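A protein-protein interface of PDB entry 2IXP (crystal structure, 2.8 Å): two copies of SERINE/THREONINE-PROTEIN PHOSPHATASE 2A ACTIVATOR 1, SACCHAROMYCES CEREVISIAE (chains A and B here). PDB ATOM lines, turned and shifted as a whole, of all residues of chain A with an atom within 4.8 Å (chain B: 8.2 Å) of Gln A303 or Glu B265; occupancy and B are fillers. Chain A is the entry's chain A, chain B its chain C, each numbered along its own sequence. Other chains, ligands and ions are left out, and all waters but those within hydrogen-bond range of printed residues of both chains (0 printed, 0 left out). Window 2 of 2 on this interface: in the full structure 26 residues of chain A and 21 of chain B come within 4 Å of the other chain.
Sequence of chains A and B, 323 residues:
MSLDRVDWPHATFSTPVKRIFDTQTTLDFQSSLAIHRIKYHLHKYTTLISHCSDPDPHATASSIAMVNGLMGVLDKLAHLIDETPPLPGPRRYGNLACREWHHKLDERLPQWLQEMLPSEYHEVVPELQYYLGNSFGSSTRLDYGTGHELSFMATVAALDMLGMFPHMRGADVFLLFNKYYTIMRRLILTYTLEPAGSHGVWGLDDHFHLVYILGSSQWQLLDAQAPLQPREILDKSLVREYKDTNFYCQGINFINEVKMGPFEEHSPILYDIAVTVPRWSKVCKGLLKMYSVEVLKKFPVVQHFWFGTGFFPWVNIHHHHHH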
ATOM      1  N   LYS A  18      -9.887  -7.218   8.697  1.00  0.00           N
ATOM      2  CA  LYS A  18     -11.255  -6.751   8.490  1.00  0.00           C
ATOM      3  C   LYS A  18     -11.703  -7.228   7.125  1.00  0.00           C
ATOM      4  O   LYS A  18     -10.917  -7.148   6.183  1.00  0.00           O
ATOM      5  CB  LYS A  18     -11.293  -5.221   8.561  1.00  0.00           C
ATOM      6  CG  LYS A  18     -12.640  -4.564   8.260  1.00  0.00           C
ATOM      7  CD  LYS A  18     -12.867  -3.349   9.150  1.00  0.00           C
ATOM      8  CE  LYS A  18     -14.228  -2.816   8.927  1.00  0.00           C
ATOM      9  NZ  LYS A  18     -15.182  -3.931   8.897  1.00  0.00           N
ATOM     10  N   ILE A  20     -15.645  -7.643   6.089  1.00  0.00           N
ATOM     11  CA  ILE A  20     -16.926  -7.026   5.766  1.00  0.00           C
ATOM     12  C   ILE A  20     -16.890  -5.498   5.806  1.00  0.00           C
ATOM     13  O   ILE A  20     -16.657  -4.874   6.843  1.00  0.00           O
ATOM     14  CB  ILE A  20     -17.950  -7.460   6.715  1.00  0.00           C
ATOM     15  CG1 ILE A  20     -18.049  -8.947   6.624  1.00  0.00           C
ATOM     16  CG2 ILE A  20     -19.264  -6.851   6.358  1.00  0.00           C
ATOM     17  CD1 ILE A  20     -18.011  -9.575   7.956  1.00  0.00           C
ATOM     18  N   ARG A 141     -15.214   1.561  21.315  1.00  0.00           N
ATOM     19  CA  ARG A 141     -16.583   2.048  21.203  1.00  0.00           C
ATOM     20  C   ARG A 141     -17.342   1.991  22.544  1.00  0.00           C
ATOM     21  O   ARG A 141     -18.342   2.677  22.688  1.00  0.00           O
ATOM     22  CB  ARG A 141     -17.316   1.270  20.125  1.00  0.00           C
ATOM     23  CG  ARG A 141     -18.384   2.020  19.348  1.00  0.00           C
ATOM     24  CD  ARG A 141     -18.920   1.084  18.215  1.00  0.00           C
ATOM     25  NE  ARG A 141     -17.809   0.357  17.564  1.00  0.00           N
ATOM     26  CZ  ARG A 141     -17.651  -0.978  17.543  1.00  0.00           C
ATOM     27  NH1 ARG A 141     -18.561  -1.795  18.109  1.00  0.00           N
ATOM     28  NH2 ARG A 141     -16.574  -1.507  16.941  1.00  0.00           N
ATOM     29  N   PHE A 299     -25.095  -5.935   8.490  1.00  0.00           N
ATOM     30  CA  PHE A 299     -23.737  -5.411   8.472  1.00  0.00           C
ATOM     31  C   PHE A 299     -23.383  -4.618   9.696  1.00  0.00           C
ATOM     32  O   PHE A 299     -22.243  -4.712  10.135  1.00  0.00           O
ATOM     33  CB  PHE A 299     -23.497  -4.589   7.195  1.00  0.00           C
ATOM     34  CG  PHE A 299     -22.484  -3.543   7.325  1.00  0.00           C
ATOM     35  CD1 PHE A 299     -21.159  -3.836   7.148  1.00  0.00           C
ATOM     36  CD2 PHE A 299     -22.858  -2.240   7.584  1.00  0.00           C
ATOM     37  CE1 PHE A 299     -20.184  -2.841   7.242  1.00  0.00           C
ATOM     38  CE2 PHE A 299     -21.912  -1.232   7.703  1.00  0.00           C
ATOM     39  CZ  PHE A 299     -20.561  -1.541   7.530  1.00  0.00           C
ATOM     40  N   PRO A 300     -24.328  -3.801  10.232  1.00  0.00           N
ATOM     41  CA  PRO A 300     -23.934  -3.044  11.393  1.00  0.00           C
ATOM     42  C   PRO A 300     -23.404  -3.973  12.434  1.00  0.00           C
ATOM     43  O   PRO A 300     -22.603  -3.509  13.264  1.00  0.00           O
ATOM     44  CB  PRO A 300     -25.234  -2.435  11.855  1.00  0.00           C
ATOM     45  CG  PRO A 300     -25.924  -2.220  10.643  1.00  0.00           C
ATOM     46  CD  PRO A 300     -25.709  -3.456   9.860  1.00  0.00           C
ATOM     47  N   VAL A 301     -23.809  -5.262  12.345  1.00  0.00           N
ATOM     48  CA  VAL A 301     -23.560  -6.312  13.334  1.00  0.00           C
ATOM     49  C   VAL A 301     -22.364  -7.206  13.007  1.00  0.00           C
ATOM     50  O   VAL A 301     -21.811  -7.792  13.900  1.00  0.00           O
ATOM     51  CB  VAL A 301     -24.859  -7.213  13.534  1.00  0.00           C
ATOM     52  CG1 VAL A 301     -24.653  -8.393  14.527  1.00  0.00           C
ATOM     53  CG2 VAL A 301     -26.038  -6.378  13.967  1.00  0.00           C
ATOM     54  N   VAL A 302     -21.981  -7.370  11.749  1.00  0.00           N
ATOM     55  CA  VAL A 302     -20.917  -8.328  11.457  1.00  0.00           C
ATOM     56  C   VAL A 302     -19.684  -7.765  10.883  1.00  0.00           C
ATOM     57  O   VAL A 302     -18.683  -8.401  10.916  1.00  0.00           O
ATOM     58  CB  VAL A 302     -21.358  -9.461  10.566  1.00  0.00           C
ATOM     59  CG1 VAL A 302     -22.112 -10.450  11.397  1.00  0.00           C
ATOM     60  CG2 VAL A 302     -22.197  -8.978   9.386  1.00  0.00           C
ATOM     61  N   GLN A 303     -19.779  -6.585  10.312  1.00  0.00           N
ATOM     62  CA  GLN A 303     -18.645  -5.716  10.005  1.00  0.00           C
ATOM     63  C   GLN A 303     -17.377  -6.048  10.787  1.00  0.00           C
ATOM     64  O   GLN A 303     -16.274  -6.174  10.216  1.00  0.00           O
ATOM     65  CB  GLN A 303     -19.086  -4.307  10.363  1.00  0.00           C
ATOM     66  CG  GLN A 303     -18.113  -3.170  10.109  1.00  0.00           C
ATOM     67  CD  GLN A 303     -18.772  -1.823  10.461  1.00  0.00           C
ATOM     68  OE1 GLN A 303     -19.856  -1.813  11.071  1.00  0.00           O
ATOM     69  NE2 GLN A 303     -18.126  -0.699  10.100  1.00  0.00           N
ATOM     70  N   HIS A 304     -17.536  -6.204  12.097  1.00  0.00           N
ATOM     71  CA  HIS A 304     -16.412  -6.408  12.974  1.00  0.00           C
ATOM     72  C   HIS A 304     -16.298  -7.849  13.256  1.00  0.00           C
ATOM     73  O   HIS A 304     -16.075  -8.215  14.364  1.00  0.00           O
ATOM     74  CB  HIS A 304     -16.610  -5.672  14.291  1.00  0.00           C
ATOM     75  CG  HIS A 304     -17.118  -4.278  14.114  1.00  0.00           C
ATOM     76  ND1 HIS A 304     -16.452  -3.331  13.351  1.00  0.00           N
ATOM     77  CD2 HIS A 304     -18.242  -3.676  14.572  1.00  0.00           C
ATOM     78  CE1 HIS A 304     -17.132  -2.201  13.372  1.00  0.00           C
ATOM     79  NE2 HIS A 304     -18.226  -2.383  14.097  1.00  0.00           N
ATOM     80  N   PHE A 305     -16.478  -8.695  12.275  1.00  0.00           N
ATOM     81  CA  PHE A 305     -16.090 -10.040  12.490  1.00  0.00           C
ATOM     82  C   PHE A 305     -14.977 -10.267  11.517  1.00  0.00           C
ATOM     83  O   PHE A 305     -15.220 -10.408  10.314  1.00  0.00           O
ATOM     84  CB  PHE A 305     -17.255 -10.995  12.264  1.00  0.00           C
ATOM     85  CG  PHE A 305     -16.887 -12.454  12.421  1.00  0.00           C
ATOM     86  CD1 PHE A 305     -17.102 -13.108  13.623  1.00  0.00           C
ATOM     87  CD2 PHE A 305     -16.326 -13.169  11.355  1.00  0.00           C
ATOM     88  CE1 PHE A 305     -16.751 -14.457  13.789  1.00  0.00           C
ATOM     89  CE2 PHE A 305     -15.979 -14.504  11.479  1.00  0.00           C
ATOM     90  CZ  PHE A 305     -16.205 -15.164  12.709  1.00  0.00           C
ATOM     91  N   TRP A 306     -13.750 -10.282  12.026  1.00  0.00           N
ATOM     92  CA  TRP A 306     -12.610 -10.399  11.132  1.00  0.00           C
ATOM     93  C   TRP A 306     -12.224 -11.842  10.794  1.00  0.00           C
ATOM     94  O   TRP A 306     -12.513 -12.757  11.550  1.00  0.00           O
ATOM     95  CB  TRP A 306     -11.416  -9.610  11.666  1.00  0.00           C
ATOM     96  CG  TRP A 306     -11.636  -8.158  11.762  1.00  0.00           C
ATOM     97  CD1 TRP A 306     -12.795  -7.466  11.509  1.00  0.00           C
ATOM     98  CD2 TRP A 306     -10.690  -7.200  12.195  1.00  0.00           C
ATOM     99  NE1 TRP A 306     -12.605  -6.113  11.715  1.00  0.00           N
ATOM    100  CE2 TRP A 306     -11.322  -5.930  12.151  1.00  0.00           C
ATOM    101  CE3 TRP A 306      -9.360  -7.284  12.609  1.00  0.00           C
ATOM    102  CZ2 TRP A 306     -10.673  -4.776  12.505  1.00  0.00           C
ATOM    103  CZ3 TRP A 306      -8.714  -6.135  12.946  1.00  0.00           C
ATOM    104  CH2 TRP A 306      -9.370  -4.897  12.899  1.00  0.00           C
ATOM    105  N   VAL B 201     -29.326   1.734  16.016  1.00  0.00           N
ATOM    106  CA  VAL B 201     -28.484   2.084  14.901  1.00  0.00           C
ATOM    107  C   VAL B 201     -29.229   2.104  13.513  1.00  0.00           C
ATOM    108  O   VAL B 201     -28.621   2.173  12.452  1.00  0.00           O
ATOM    109  CB  VAL B 201     -27.362   1.005  14.946  1.00  0.00           C
ATOM    110  CG1 VAL B 201     -27.596  -0.144  13.943  1.00  0.00           C
ATOM    111  CG2 VAL B 201     -26.021   1.609  14.833  1.00  0.00           C
ATOM    112  N   LYS B 259     -21.814   9.572  22.952  1.00  0.00           N
ATOM    113  CA  LYS B 259     -21.607   8.280  22.324  1.00  0.00           C
ATOM    114  C   LYS B 259     -20.162   8.169  21.878  1.00  0.00           C
ATOM    115  O   LYS B 259     -19.592   9.119  21.364  1.00  0.00           O
ATOM    116  CB  LYS B 259     -22.565   8.143  21.139  1.00  0.00           C
ATOM    117  CG  LYS B 259     -23.935   7.460  21.398  1.00  0.00           C
ATOM    118  CD  LYS B 259     -24.817   7.729  20.181  1.00  0.00           C
ATOM    119  CE  LYS B 259     -26.084   6.887  20.116  1.00  0.00           C
ATOM    120  NZ  LYS B 259     -25.868   5.528  19.583  1.00  0.00           N
ATOM    121  N   MET B 260     -19.569   7.004  22.041  1.00  0.00           N
ATOM    122  CA  MET B 260     -18.150   6.967  22.170  1.00  0.00           C
ATOM    123  C   MET B 260     -17.297   6.661  20.956  1.00  0.00           C
ATOM    124  O   MET B 260     -16.123   7.022  20.956  1.00  0.00           O
ATOM    125  CB  MET B 260     -17.792   5.987  23.262  1.00  0.00           C
ATOM    126  CG  MET B 260     -16.520   6.349  24.045  1.00  0.00           C
ATOM    127  SD  MET B 260     -16.803   7.555  25.385  1.00  0.00           S
ATOM    128  CE  MET B 260     -18.583   7.333  25.843  1.00  0.00           C
ATOM    129  N   GLY B 261     -17.824   5.980  19.946  1.00  0.00           N
ATOM    130  CA  GLY B 261     -16.946   5.459  18.864  1.00  0.00           C
ATOM    131  C   GLY B 261     -16.610   6.409  17.720  1.00  0.00           C
ATOM    132  O   GLY B 261     -16.757   7.591  17.845  1.00  0.00           O
ATOM    133  N   PRO B 262     -16.131   5.887  16.591  1.00  0.00           N
ATOM    134  CA  PRO B 262     -16.157   6.720  15.405  1.00  0.00           C
ATOM    135  C   PRO B 262     -17.595   6.997  15.027  1.00  0.00           C
ATOM    136  O   PRO B 262     -18.391   6.095  15.010  1.00  0.00           O
ATOM    137  CB  PRO B 262     -15.508   5.839  14.336  1.00  0.00           C
ATOM    138  CG  PRO B 262     -14.722   4.779  15.111  1.00  0.00           C
ATOM    139  CD  PRO B 262     -15.523   4.564  16.348  1.00  0.00           C
ATOM    140  N   PHE B 263     -17.912   8.252  14.725  1.00  0.00           N
ATOM    141  CA  PHE B 263     -19.280   8.687  14.432  1.00  0.00           C
ATOM    142  C   PHE B 263     -19.976   7.805  13.431  1.00  0.00           C
ATOM    143  O   PHE B 263     -21.138   7.485  13.627  1.00  0.00           O
ATOM    144  CB  PHE B 263     -19.326  10.137  13.958  1.00  0.00           C
ATOM    145  CG  PHE B 263     -20.709  10.669  13.763  1.00  0.00           C
ATOM    146  CD1 PHE B 263     -21.388  11.285  14.803  1.00  0.00           C
ATOM    147  CD2 PHE B 263     -21.343  10.604  12.502  1.00  0.00           C
ATOM    148  CE1 PHE B 263     -22.706  11.821  14.593  1.00  0.00           C
ATOM    149  CE2 PHE B 263     -22.656  11.157  12.283  1.00  0.00           C
ATOM    150  CZ  PHE B 263     -23.336  11.740  13.340  1.00  0.00           C
ATOM    151  N   GLU B 264     -19.287   7.407  12.372  1.00  0.00           N
ATOM    152  CA  GLU B 264     -19.855   6.596  11.299  1.00  0.00           C
ATOM    153  C   GLU B 264     -20.423   5.233  11.749  1.00  0.00           C
ATOM    154  O   GLU B 264     -21.392   4.741  11.173  1.00  0.00           O
ATOM    155  CB  GLU B 264     -18.749   6.433  10.302  1.00  0.00           C
ATOM    156  CG  GLU B 264     -18.945   5.605   9.100  1.00  0.00           C
ATOM    157  CD  GLU B 264     -17.630   5.549   8.362  1.00  0.00           C
ATOM    158  OE1 GLU B 264     -16.710   6.340   8.738  1.00  0.00           O
ATOM    159  OE2 GLU B 264     -17.490   4.719   7.433  1.00  0.00           O
ATOM    160  N   GLU B 265     -19.839   4.654  12.796  1.00  0.00           N
ATOM    161  CA  GLU B 265     -20.247   3.341  13.342  1.00  0.00           C
ATOM    162  C   GLU B 265     -21.481   3.436  14.205  1.00  0.00           C
ATOM    163  O   GLU B 265     -22.241   2.464  14.295  1.00  0.00           O
ATOM    164  CB  GLU B 265     -19.173   2.727  14.206  1.00  0.00           C
ATOM    165  CG  GLU B 265     -18.599   1.553  13.581  1.00  0.00           C
ATOM    166  CD  GLU B 265     -17.105   1.701  13.103  1.00  0.00           C
ATOM    167  OE1 GLU B 265     -16.147   1.437  13.895  1.00  0.00           O
ATOM    168  OE2 GLU B 265     -16.882   1.987  11.896  1.00  0.00           O
ATOM    169  N   HIS B 266     -21.703   4.591  14.831  1.00  0.00           N
ATOM    170  CA  HIS B 266     -22.771   4.666  15.797  1.00  0.00           C
ATOM    171  C   HIS B 266     -23.963   5.439  15.304  1.00  0.00           C
ATOM    172  O   HIS B 266     -25.061   5.281  15.838  1.00  0.00           O
ATOM    173  CB  HIS B 266     -22.320   5.164  17.187  1.00  0.00           C
ATOM    174  CG  HIS B 266     -21.890   6.606  17.247  1.00  0.00           C
ATOM    175  ND1 HIS B 266     -20.585   6.988  17.539  1.00  0.00           N
ATOM    176  CD2 HIS B 266     -22.597   7.754  17.108  1.00  0.00           C
ATOM    177  CE1 HIS B 266     -20.507   8.307  17.538  1.00  0.00           C
ATOM    178  NE2 HIS B 266     -21.713   8.795  17.272  1.00  0.00           N
ATOM    179  N   SER B 267     -23.790   6.275  14.294  1.00  0.00           N
ATOM    180  CA  SER B 267     -24.912   7.072  13.861  1.00  0.00           C
ATOM    181  C   SER B 267     -24.897   6.883  12.378  1.00  0.00           C
ATOM    182  O   SER B 267     -24.740   7.831  11.603  1.00  0.00           O
ATOM    183  CB  SER B 267     -24.698   8.510  14.310  1.00  0.00           C
ATOM    184  OG  SER B 267     -24.878   8.575  15.715  1.00  0.00           O
ATOM    185  N   PRO B 268     -24.989   5.624  11.949  1.00  0.00           N
ATOM    186  CA  PRO B 268     -24.852   5.422  10.530  1.00  0.00           C
ATOM    187  C   PRO B 268     -25.816   6.229   9.655  1.00  0.00           C
ATOM    188  O   PRO B 268     -25.400   6.678   8.649  1.00  0.00           O
ATOM    189  CB  PRO B 268     -25.021   3.915  10.358  1.00  0.00           C
ATOM    190  CG  PRO B 268     -25.568   3.476  11.559  1.00  0.00           C
ATOM    191  CD  PRO B 268     -25.186   4.368  12.651  1.00  0.00           C
ATOM    192  N   ILE B 269     -27.068   6.435  10.001  1.00  0.00           N
ATOM    193  CA  ILE B 269     -27.924   7.221   9.125  1.00  0.00           C
ATOM    194  C   ILE B 269     -27.457   8.678   9.023  1.00  0.00           C
ATOM    195  O   ILE B 269     -27.133   9.167   7.923  1.00  0.00           O
ATOM    196  CB  ILE B 269     -29.389   7.156   9.608  1.00  0.00           C
ATOM    197  CG1 ILE B 269     -29.996   5.824   9.188  1.00  0.00           C
ATOM    198  CG2 ILE B 269     -30.257   8.331   9.063  1.00  0.00           C
ATOM    199  CD1 ILE B 269     -30.909   5.310  10.226  1.00  0.00           C
ATOM    200  N   TYR B 271     -24.722   9.660   9.445  1.00  0.00           N
ATOM    201  CA  TYR B 271     -23.514   9.643   8.641  1.00  0.00           C
ATOM    202  C   TYR B 271     -23.813   9.663   7.111  1.00  0.00           C
ATOM    203  O   TYR B 271     -23.378  10.579   6.396  1.00  0.00           O
ATOM    204  CB  TYR B 271     -22.583   8.518   9.046  1.00  0.00           C
ATOM    205  CG  TYR B 271     -21.353   8.496   8.205  1.00  0.00           C
ATOM    206  CD1 TYR B 271     -20.148   8.947   8.702  1.00  0.00           C
ATOM    207  CD2 TYR B 271     -21.389   8.052   6.892  1.00  0.00           C
ATOM    208  CE1 TYR B 271     -18.980   8.924   7.909  1.00  0.00           C
ATOM    209  CE2 TYR B 271     -20.248   8.035   6.102  1.00  0.00           C
ATOM    210  CZ  TYR B 271     -19.036   8.459   6.604  1.00  0.00           C
ATOM    211  OH  TYR B 271     -17.893   8.438   5.807  1.00  0.00           O
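NE2 of Gln A303 lies within hydrogen-bond range of OE2 of Glu B265 (3.5 Å).
Of the 13 printed residues of chain B, 4 touch a printed residue of chain A.
Hydrophobic or aromatic side chains of chain A that line the printed part of chain B: Pro A300 and His A304.
Among the printed residues, no Asp or Glu carboxylate lies within 4 Å of a Lys or Arg side-chain nitrogen of the other chain.
The guanidinium group of Arg A141 is in hydrogen-bond range of a ring nitrogen (NE2) of His A304, at 3.4 Å.
The side-chain amide oxygen (OE1) of Gln A303 sits at hydrogen-bond distance from a ring nitrogen (NE2) of His A304 (3.5 Å).
NZ of Lys A18 is in hydrogen-bond range of O of Gln A303.
No position is printed for both chains.
Of the 5 pairs that touch across the chains among the printed residues, none has its exchanged pair printed and touching as well.
O of Arg A141 touches CB of Met B260, 3.4 Å away.
CG of Arg A141 touches CA of Gly B261 (3.8 Å).
Val B201 touches Pro A300.
Glu B265 touches His A304.
Of chain B, only Glu B265 comes within 4 Å of Gln A303.
Of the printed residues of chain A, Gly B261 touches Arg A141.
Printed residues of chain B within 4 Å of His A304: Glu B265 (3.8 Å).
Phe A305 touches none of the printed residues of chain B.
The nearest residue of chain B that does not touch Gln A303 is Glu B264 (6.1 Å).
The nearest printed residue of chain B that does not touch His A304 is Pro B262 (7.6 Å).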
